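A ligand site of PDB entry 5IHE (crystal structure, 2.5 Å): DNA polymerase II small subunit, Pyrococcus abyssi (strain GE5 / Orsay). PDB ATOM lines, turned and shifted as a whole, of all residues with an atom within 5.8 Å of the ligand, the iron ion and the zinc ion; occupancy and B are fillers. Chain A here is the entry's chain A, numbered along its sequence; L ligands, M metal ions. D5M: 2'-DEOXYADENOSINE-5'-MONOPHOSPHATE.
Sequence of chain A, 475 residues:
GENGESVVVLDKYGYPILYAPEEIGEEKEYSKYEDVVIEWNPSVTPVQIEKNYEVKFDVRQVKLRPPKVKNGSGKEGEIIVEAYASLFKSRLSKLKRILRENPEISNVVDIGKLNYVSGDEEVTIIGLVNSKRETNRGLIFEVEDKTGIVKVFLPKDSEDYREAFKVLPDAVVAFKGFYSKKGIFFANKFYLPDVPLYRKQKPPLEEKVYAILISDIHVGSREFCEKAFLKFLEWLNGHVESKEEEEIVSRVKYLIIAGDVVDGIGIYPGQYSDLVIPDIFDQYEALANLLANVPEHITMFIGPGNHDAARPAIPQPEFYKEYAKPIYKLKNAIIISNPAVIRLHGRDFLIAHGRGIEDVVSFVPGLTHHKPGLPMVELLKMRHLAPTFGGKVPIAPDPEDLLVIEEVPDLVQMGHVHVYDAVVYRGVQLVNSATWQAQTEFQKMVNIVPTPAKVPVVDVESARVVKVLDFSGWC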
ATOM      1  N   ASP A 216      -0.435   0.338 -15.840  1.00  0.00           N
ATOM      2  CA  ASP A 216      -0.614   0.120 -14.408  1.00  0.00           C
ATOM      3  C   ASP A 216      -0.088  -1.234 -13.962  1.00  0.00           C
ATOM      4  O   ASP A 216      -0.824  -2.065 -13.409  1.00  0.00           O
ATOM      5  CB  ASP A 216      -2.069   0.377 -14.009  1.00  0.00           C
ATOM      6  CG  ASP A 216      -2.514   1.779 -14.335  1.00  0.00           C
ATOM      7  OD1 ASP A 216      -2.511   2.627 -13.415  1.00  0.00           O
ATOM      8  OD2 ASP A 216      -2.819   2.049 -15.519  1.00  0.00           O
ATOM      9  N   HIS A 218       2.383  -1.599 -11.711  1.00  0.00           N
ATOM     10  CA  HIS A 218       2.537  -1.409 -10.271  1.00  0.00           C
ATOM     11  C   HIS A 218       3.535  -2.367  -9.633  1.00  0.00           C
ATOM     12  O   HIS A 218       3.254  -2.935  -8.577  1.00  0.00           O
ATOM     13  CB  HIS A 218       1.168  -1.445  -9.547  1.00  0.00           C
ATOM     14  CG  HIS A 218       0.340  -0.235  -9.789  1.00  0.00           C
ATOM     15  ND1 HIS A 218       0.444   0.878  -8.996  1.00  0.00           N
ATOM     16  CD2 HIS A 218      -0.545   0.016 -10.780  1.00  0.00           C
ATOM     17  CE1 HIS A 218      -0.393   1.772  -9.499  1.00  0.00           C
ATOM     18  NE2 HIS A 218      -1.003   1.301 -10.582  1.00  0.00           N
ATOM     19  N   GLY A 259       1.748   4.336 -18.200  1.00  0.00           N
ATOM     20  CA  GLY A 259       1.867   4.758 -16.810  1.00  0.00           C
ATOM     21  C   GLY A 259       1.681   3.754 -15.702  1.00  0.00           C
ATOM     22  O   GLY A 259       1.179   2.650 -15.916  1.00  0.00           O
ATOM     23  N   ASP A 260       2.065   4.191 -14.460  1.00  0.00           N
ATOM     24  CA  ASP A 260       2.094   3.467 -13.188  1.00  0.00           C
ATOM     25  C   ASP A 260       2.819   2.123 -13.338  1.00  0.00           C
ATOM     26  O   ASP A 260       2.313   1.069 -12.964  1.00  0.00           O
ATOM     27  CB  ASP A 260       0.703   3.350 -12.565  1.00  0.00           C
ATOM     28  CG  ASP A 260       0.147   4.652 -12.037  1.00  0.00           C
ATOM     29  OD1 ASP A 260       0.921   5.578 -11.809  1.00  0.00           O
ATOM     30  OD2 ASP A 260      -1.076   4.751 -11.873  1.00  0.00           O
ATOM     31  N   ILE A 267       2.983   7.469  -2.040  1.00  0.00           N
ATOM     32  CA  ILE A 267       1.873   7.909  -2.920  1.00  0.00           C
ATOM     33  C   ILE A 267       0.606   8.202  -2.093  1.00  0.00           C
ATOM     34  O   ILE A 267      -0.080   9.204  -2.337  1.00  0.00           O
ATOM     35  CB  ILE A 267       1.652   6.913  -4.104  1.00  0.00           C
ATOM     36  CG1 ILE A 267       2.956   6.670  -4.915  1.00  0.00           C
ATOM     37  CG2 ILE A 267       0.498   7.332  -5.020  1.00  0.00           C
ATOM     38  CD1 ILE A 267       3.693   7.929  -5.501  1.00  0.00           C
ATOM     39  N   GLY A 305       3.172   7.558 -15.058  1.00  0.00           N
ATOM     40  CA  GLY A 305       1.875   7.690 -14.394  1.00  0.00           C
ATOM     41  C   GLY A 305       2.039   8.474 -13.101  1.00  0.00           C
ATOM     42  O   GLY A 305       3.121   9.002 -12.847  1.00  0.00           O
ATOM     43  N   ASN A 306       1.006   8.529 -12.245  1.00  0.00           N
ATOM     44  CA  ASN A 306       1.087   9.278 -10.982  1.00  0.00           C
ATOM     45  C   ASN A 306       1.831   8.558  -9.828  1.00  0.00           C
ATOM     46  O   ASN A 306       2.140   9.200  -8.831  1.00  0.00           O
ATOM     47  CB  ASN A 306      -0.306   9.743 -10.516  1.00  0.00           C
ATOM     48  CG  ASN A 306      -1.311   8.636 -10.376  1.00  0.00           C
ATOM     49  OD1 ASN A 306      -1.691   7.986 -11.350  1.00  0.00           O
ATOM     50  ND2 ASN A 306      -1.779   8.415  -9.153  1.00  0.00           N
ATOM     51  N   HIS A 307       2.123   7.260  -9.971  1.00  0.00           N
ATOM     52  CA  HIS A 307       2.854   6.480  -8.952  1.00  0.00           C
ATOM     53  C   HIS A 307       4.334   6.501  -9.251  1.00  0.00           C
ATOM     54  O   HIS A 307       5.155   6.248  -8.373  1.00  0.00           O
ATOM     55  CB  HIS A 307       2.360   5.021  -8.909  1.00  0.00           C
ATOM     56  CG  HIS A 307       1.067   4.833  -8.159  1.00  0.00           C
ATOM     57  ND1 HIS A 307       1.005   4.032  -7.041  1.00  0.00           N
ATOM     58  CD2 HIS A 307      -0.150   5.362  -8.395  1.00  0.00           C
ATOM     59  CE1 HIS A 307      -0.254   4.090  -6.625  1.00  0.00           C
ATOM     60  NE2 HIS A 307      -0.984   4.870  -7.405  1.00  0.00           N
ATOM     61  N   HIS A 353      -1.911   8.909 -19.359  1.00  0.00           N
ATOM     62  CA  HIS A 353      -2.109   8.031 -18.214  1.00  0.00           C
ATOM     63  C   HIS A 353      -3.571   7.849 -17.863  1.00  0.00           C
ATOM     64  O   HIS A 353      -3.981   6.739 -17.556  1.00  0.00           O
ATOM     65  CB  HIS A 353      -1.280   8.425 -16.999  1.00  0.00           C
ATOM     66  CG  HIS A 353      -1.410   7.446 -15.873  1.00  0.00           C
ATOM     67  ND1 HIS A 353      -1.164   6.097 -16.058  1.00  0.00           N
ATOM     68  CD2 HIS A 353      -1.808   7.640 -14.601  1.00  0.00           C
ATOM     69  CE1 HIS A 353      -1.416   5.516 -14.907  1.00  0.00           C
ATOM     70  NE2 HIS A 353      -1.813   6.405 -13.998  1.00  0.00           N
ATOM     71  N   ARG A 355      -5.608  10.546 -15.997  1.00  0.00           N
ATOM     72  CA  ARG A 355      -6.006  11.382 -14.869  1.00  0.00           C
ATOM     73  C   ARG A 355      -7.340  12.080 -15.095  1.00  0.00           C
ATOM     74  O   ARG A 355      -8.122  12.238 -14.148  1.00  0.00           O
ATOM     75  CB  ARG A 355      -4.896  12.389 -14.479  1.00  0.00           C
ATOM     76  CG  ARG A 355      -3.567  11.781 -13.987  1.00  0.00           C
ATOM     77  CD  ARG A 355      -3.639  10.824 -12.784  1.00  0.00           C
ATOM     78  NE  ARG A 355      -4.352  11.375 -11.622  1.00  0.00           N
ATOM     79  CZ  ARG A 355      -3.789  12.137 -10.677  1.00  0.00           C
ATOM     80  NH1 ARG A 355      -2.498  12.452 -10.745  1.00  0.00           N
ATOM     81  NH2 ARG A 355      -4.520  12.585  -9.676  1.00  0.00           N
ATOM     82  N   GLU A 358     -10.920  10.475 -14.073  1.00  0.00           N
ATOM     83  CA  GLU A 358     -11.359  10.775 -12.701  1.00  0.00           C
ATOM     84  C   GLU A 358     -12.156  12.060 -12.652  1.00  0.00           C
ATOM     85  O   GLU A 358     -13.168  12.101 -11.966  1.00  0.00           O
ATOM     86  CB  GLU A 358     -10.175  10.880 -11.741  1.00  0.00           C
ATOM     87  CG  GLU A 358      -9.827   9.546 -11.103  1.00  0.00           C
ATOM     88  CD  GLU A 358      -8.964   9.566  -9.862  1.00  0.00           C
ATOM     89  OE1 GLU A 358      -7.899  10.209  -9.891  1.00  0.00           O
ATOM     90  OE2 GLU A 358      -9.501   9.171  -8.796  1.00  0.00           O
ATOM     91  N   HIS A 369     -16.649   4.495 -13.372  1.00  0.00           N
ATOM     92  CA  HIS A 369     -15.698   3.453 -13.773  1.00  0.00           C
ATOM     93  C   HIS A 369     -16.562   2.185 -14.024  1.00  0.00           C
ATOM     94  O   HIS A 369     -17.789   2.313 -14.107  1.00  0.00           O
ATOM     95  CB  HIS A 369     -14.518   3.288 -12.771  1.00  0.00           C
ATOM     96  CG  HIS A 369     -14.770   2.437 -11.565  1.00  0.00           C
ATOM     97  ND1 HIS A 369     -13.930   1.366 -11.250  1.00  0.00           N
ATOM     98  CD2 HIS A 369     -15.713   2.538 -10.600  1.00  0.00           C
ATOM     99  CE1 HIS A 369     -14.411   0.836 -10.130  1.00  0.00           C
ATOM    100  NE2 HIS A 369     -15.479   1.509  -9.705  1.00  0.00           N
ATOM    101  N   LYS A 392      -7.078  15.809  -7.254  1.00  0.00           N
ATOM    102  CA  LYS A 392      -5.785  15.250  -6.849  1.00  0.00           C
ATOM    103  C   LYS A 392      -4.893  15.349  -8.104  1.00  0.00           C
ATOM    104  O   LYS A 392      -3.683  15.154  -8.006  1.00  0.00           O
ATOM    105  CB  LYS A 392      -5.908  13.791  -6.362  1.00  0.00           C
ATOM    106  CG  LYS A 392      -6.674  13.614  -5.050  1.00  0.00           C
ATOM    107  CD  LYS A 392      -8.124  13.200  -5.297  1.00  0.00           C
ATOM    108  CE  LYS A 392      -8.734  12.435  -4.147  1.00  0.00           C
ATOM    109  NZ  LYS A 392     -10.136  12.053  -4.434  1.00  0.00           N
ATOM    110  N   HIS A 416      -4.624   4.285 -15.687  1.00  0.00           N
ATOM    111  CA  HIS A 416      -5.017   4.921 -14.426  1.00  0.00           C
ATOM    112  C   HIS A 416      -6.219   4.290 -13.711  1.00  0.00           C
ATOM    113  O   HIS A 416      -6.073   4.031 -12.526  1.00  0.00           O
ATOM    114  CB  HIS A 416      -5.231   6.444 -14.594  1.00  0.00           C
ATOM    115  CG  HIS A 416      -5.510   7.167 -13.322  1.00  0.00           C
ATOM    116  ND1 HIS A 416      -4.597   7.184 -12.284  1.00  0.00           N
ATOM    117  CD2 HIS A 416      -6.591   7.889 -12.955  1.00  0.00           C
ATOM    118  CE1 HIS A 416      -5.153   7.902 -11.315  1.00  0.00           C
ATOM    119  NE2 HIS A 416      -6.349   8.343 -11.681  1.00  0.00           N
ATOM    120  N   VAL A 417      -7.399   4.104 -14.348  1.00  0.00           N
ATOM    121  CA  VAL A 417      -8.601   3.636 -13.632  1.00  0.00           C
ATOM    122  C   VAL A 417      -8.628   2.117 -13.287  1.00  0.00           C
ATOM    123  O   VAL A 417      -9.470   1.713 -12.462  1.00  0.00           O
ATOM    124  CB  VAL A 417      -9.930   4.063 -14.303  1.00  0.00           C
ATOM    125  CG1 VAL A 417      -9.981   5.576 -14.459  1.00  0.00           C
ATOM    126  CG2 VAL A 417     -10.152   3.364 -15.634  1.00  0.00           C
ATOM    127  N   HIS A 418      -7.731   1.315 -13.881  1.00  0.00           N
ATOM    128  CA  HIS A 418      -7.559  -0.133 -13.620  1.00  0.00           C
ATOM    129  C   HIS A 418      -8.719  -1.010 -14.124  1.00  0.00           C
ATOM    130  O   HIS A 418      -8.802  -2.183 -13.744  1.00  0.00           O
ATOM    131  CB  HIS A 418      -7.291  -0.392 -12.117  1.00  0.00           C
ATOM    132  CG  HIS A 418      -5.949   0.091 -11.643  1.00  0.00           C
ATOM    133  ND1 HIS A 418      -5.390  -0.393 -10.482  1.00  0.00           N
ATOM    134  CD2 HIS A 418      -5.101   0.980 -12.191  1.00  0.00           C
ATOM    135  CE1 HIS A 418      -4.224   0.204 -10.356  1.00  0.00           C
ATOM    136  NE2 HIS A 418      -4.008   1.044 -11.363  1.00  0.00           N
ATOM    137  N   THR A 435      -4.905  -2.944 -15.843  1.00  0.00           N
ATOM    138  CA  THR A 435      -3.835  -3.033 -14.838  1.00  0.00           C
ATOM    139  C   THR A 435      -3.284  -4.464 -14.681  1.00  0.00           C
ATOM    140  O   THR A 435      -3.917  -5.432 -15.111  1.00  0.00           O
ATOM    141  CB  THR A 435      -4.396  -2.552 -13.463  1.00  0.00           C
ATOM    142  OG1 THR A 435      -3.357  -2.450 -12.507  1.00  0.00           O
ATOM    143  CG2 THR A 435      -5.527  -3.442 -12.918  1.00  0.00           C
ATOM    144  N   GLN A 437      -2.355  -5.096 -11.460  1.00  0.00           N
ATOM    145  CA  GLN A 437      -2.497  -5.014 -10.007  1.00  0.00           C
ATOM    146  C   GLN A 437      -3.889  -5.418  -9.566  1.00  0.00           C
ATOM    147  O   GLN A 437      -4.862  -4.812  -9.990  1.00  0.00           O
ATOM    148  CB  GLN A 437      -2.160  -3.587  -9.527  1.00  0.00           C
ATOM    149  CG  GLN A 437      -2.313  -3.401  -8.015  1.00  0.00           C
ATOM    150  CD  GLN A 437      -2.010  -2.020  -7.499  1.00  0.00           C
ATOM    151  OE1 GLN A 437      -2.656  -1.026  -7.868  1.00  0.00           O
ATOM    152  NE2 GLN A 437      -1.079  -1.945  -6.588  1.00  0.00           N
ATOM    153  N   PHE A 442      -6.486  -0.193   0.059  1.00  0.00           N
ATOM    154  CA  PHE A 442      -6.922   1.176  -0.223  1.00  0.00           C
ATOM    155  C   PHE A 442      -8.011   1.246  -1.281  1.00  0.00           C
ATOM    156  O   PHE A 442      -8.972   2.000  -1.089  1.00  0.00           O
ATOM    157  CB  PHE A 442      -5.728   2.060  -0.588  1.00  0.00           C
ATOM    158  CG  PHE A 442      -5.999   3.531  -0.445  1.00  0.00           C
ATOM    159  CD1 PHE A 442      -6.356   4.301  -1.549  1.00  0.00           C
ATOM    160  CD2 PHE A 442      -5.932   4.152   0.798  1.00  0.00           C
ATOM    161  CE1 PHE A 442      -6.634   5.661  -1.414  1.00  0.00           C
ATOM    162  CE2 PHE A 442      -6.185   5.526   0.925  1.00  0.00           C
ATOM    163  CZ  PHE A 442      -6.537   6.260  -0.188  1.00  0.00           C
ATOM    164  N   GLN A 443      -7.873   0.473  -2.392  1.00  0.00           N
ATOM    165  CA  GLN A 443      -8.852   0.389  -3.488  1.00  0.00           C
ATOM    166  C   GLN A 443     -10.207  -0.123  -2.958  1.00  0.00           C
ATOM    167  O   GLN A 443     -11.234   0.455  -3.281  1.00  0.00           O
ATOM    168  CB  GLN A 443      -8.329  -0.485  -4.641  1.00  0.00           C
ATOM    169  CG  GLN A 443      -7.249   0.199  -5.511  1.00  0.00           C
ATOM    170  CD  GLN A 443      -6.394  -0.749  -6.347  1.00  0.00           C
ATOM    171  OE1 GLN A 443      -6.600  -1.956  -6.424  1.00  0.00           O
ATOM    172  NE2 GLN A 443      -5.392  -0.211  -7.014  1.00  0.00           N
ATOM    173  N   VAL A 446     -11.974   2.734  -1.068  1.00  0.00           N
ATOM    174  CA  VAL A 446     -12.477   3.799  -1.942  1.00  0.00           C
ATOM    175  C   VAL A 446     -13.393   3.223  -3.061  1.00  0.00           C
ATOM    176  O   VAL A 446     -13.753   3.929  -4.014  1.00  0.00           O
ATOM    177  CB  VAL A 446     -11.358   4.748  -2.478  1.00  0.00           C
ATOM    178  CG1 VAL A 446     -10.658   5.475  -1.338  1.00  0.00           C
ATOM    179  CG2 VAL A 446     -10.350   4.006  -3.365  1.00  0.00           C
ATOM    180  N   ILE A 448     -12.883   0.846  -5.500  1.00  0.00           N
ATOM    181  CA  ILE A 448     -12.327   0.631  -6.839  1.00  0.00           C
ATOM    182  C   ILE A 448     -12.174  -0.880  -7.061  1.00  0.00           C
ATOM    183  O   ILE A 448     -11.486  -1.558  -6.279  1.00  0.00           O
ATOM    184  CB  ILE A 448     -11.018   1.463  -7.121  1.00  0.00           C
ATOM    185  CG1 ILE A 448     -11.342   2.867  -7.710  1.00  0.00           C
ATOM    186  CG2 ILE A 448     -10.049   0.736  -8.092  1.00  0.00           C
ATOM    187  CD1 ILE A 448     -11.784   3.921  -6.763  1.00  0.00           C
HETATM  188  O5' D5M L   1      -5.574   4.566  -9.492  1.00  0.00           O
HETATM  189  C5' D5M L   1      -6.422   3.384  -9.581  1.00  0.00           C
HETATM  190  C4' D5M L   1      -7.875   3.769  -9.345  1.00  0.00           C
HETATM  191  O4' D5M L   1      -8.022   4.302  -8.020  1.00  0.00           O
HETATM  192  C3' D5M L   1      -8.489   4.799 -10.293  1.00  0.00           C
HETATM  193  O3' D5M L   1      -9.827   4.429 -10.639  1.00  0.00           O
HETATM  194  C2' D5M L   1      -8.468   6.085  -9.478  1.00  0.00           C
HETATM  195  C1' D5M L   1      -8.668   5.570  -8.072  1.00  0.00           C
HETATM  196  N9  D5M L   1      -8.126   6.403  -6.995  1.00  0.00           N
HETATM  197  C8  D5M L   1      -6.798   6.661  -6.753  1.00  0.00           C
HETATM  198  N7  D5M L   1      -6.580   7.337  -5.652  1.00  0.00           N
HETATM  199  C5  D5M L   1      -7.858   7.554  -5.147  1.00  0.00           C
HETATM  200  C6  D5M L   1      -8.308   8.206  -3.987  1.00  0.00           C
HETATM  201  N6  D5M L   1      -7.503   8.815  -3.115  1.00  0.00           N
HETATM  202  N1  D5M L   1      -9.646   8.222  -3.759  1.00  0.00           N
HETATM  203  C2  D5M L   1     -10.461   7.636  -4.643  1.00  0.00           C
HETATM  204  N3  D5M L   1     -10.145   7.001  -5.782  1.00  0.00           N
HETATM  205  C4  D5M L   1      -8.821   6.988  -5.975  1.00  0.00           C
HETATM  206  P   D5M L   1      -4.018   4.575  -9.062  1.00  0.00           P
HETATM  207  O1P D5M L   1      -3.247   4.203 -10.318  1.00  0.00           O
HETATM  208  O3P D5M L   1      -3.758   3.435  -8.059  1.00  0.00           O
HETATM  209  O2P D5M L   1      -3.733   5.931  -8.435  1.00  0.00           O
HETATM  210 FE    FE M   1      -2.496   2.682 -11.484  1.00  0.00          FE
HETATM  211 ZN    ZN M   2      -2.651   6.138 -11.875  1.00  0.00          ZN
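Of the 22 residues printed, 5 come within 4 Å of the zinc ion. The nearest printed residue that does not touch the zinc ion is His 307 (4.4 Å).
A ring nitrogen (NE2) of His 307 sits at hydrogen-bond distance from an oxygen (O2P) of the ligand. O of Val 417 sits at hydrogen-bond distance from O3' of the ligand (3.3 Å).
The zinc ion is bound by OD2 of Asp 260 (2.1 Å), OD1 of Asn 306 (2.1 Å), ND1 of His 416 (2.2 Å), NE2 of His 353 (2.3 Å) and O1P of the ligand (2.6 Å). The zinc ion has five donor atoms within binding distance.
Residues that only touch the ligand: Glu 358, Lys 392, Phe 442, Val 446 and Ile 448. Within 4 Å of the ligand: Asp 216, His 218, Asp 260, Asn 306, His 307, Glu 358, Lys 392, His 416, Val 417, His 418, Phe 442, Val 446 and Ile 448.
The backbone NH (N) of His 416 is in hydrogen-bond range of the side-chain carboxylate (OD2) of Asp 216 (2.9 Å). O of Asp 216 sits at hydrogen-bond distance from OG1 of Thr 435, at 2.7 Å. N of Asp 216 lies within hydrogen-bond range of O of Gly 259. The backbone NH (N) of His 307 lies within hydrogen-bond range of the side-chain carboxylate (OD1) of Asp 260 (2.8 Å). ND1 of His 418 sits at hydrogen-bond distance from NE2 of Gln 443, 3.5 Å away. NE2 of His 416 lies within hydrogen-bond range of OE1 of Glu 358 (3.0 Å). The backbone carbonyl oxygen of Gln 443 sits at hydrogen-bond distance from the backbone NH of Ile 448 (2.8 Å). O of Lys 392 lies within hydrogen-bond range of NH2 of Arg 355.
The iron ion is bound by the side-chain carboxylate of Asp 216 (1.9 Å), an oxygen (O1P) of the ligand (2.1 Å), a ring nitrogen (NE2) of His 218 (2.2 Å), a ring nitrogen (NE2) of His 418 (2.2 Å) and the side-chain carboxylate of Asp 260 (2.5 Å). The iron ion has five donor atoms within binding distance.
Within 4 Å of the iron ion: Asp 216, His 218, Asp 260, His 416 and His 418.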
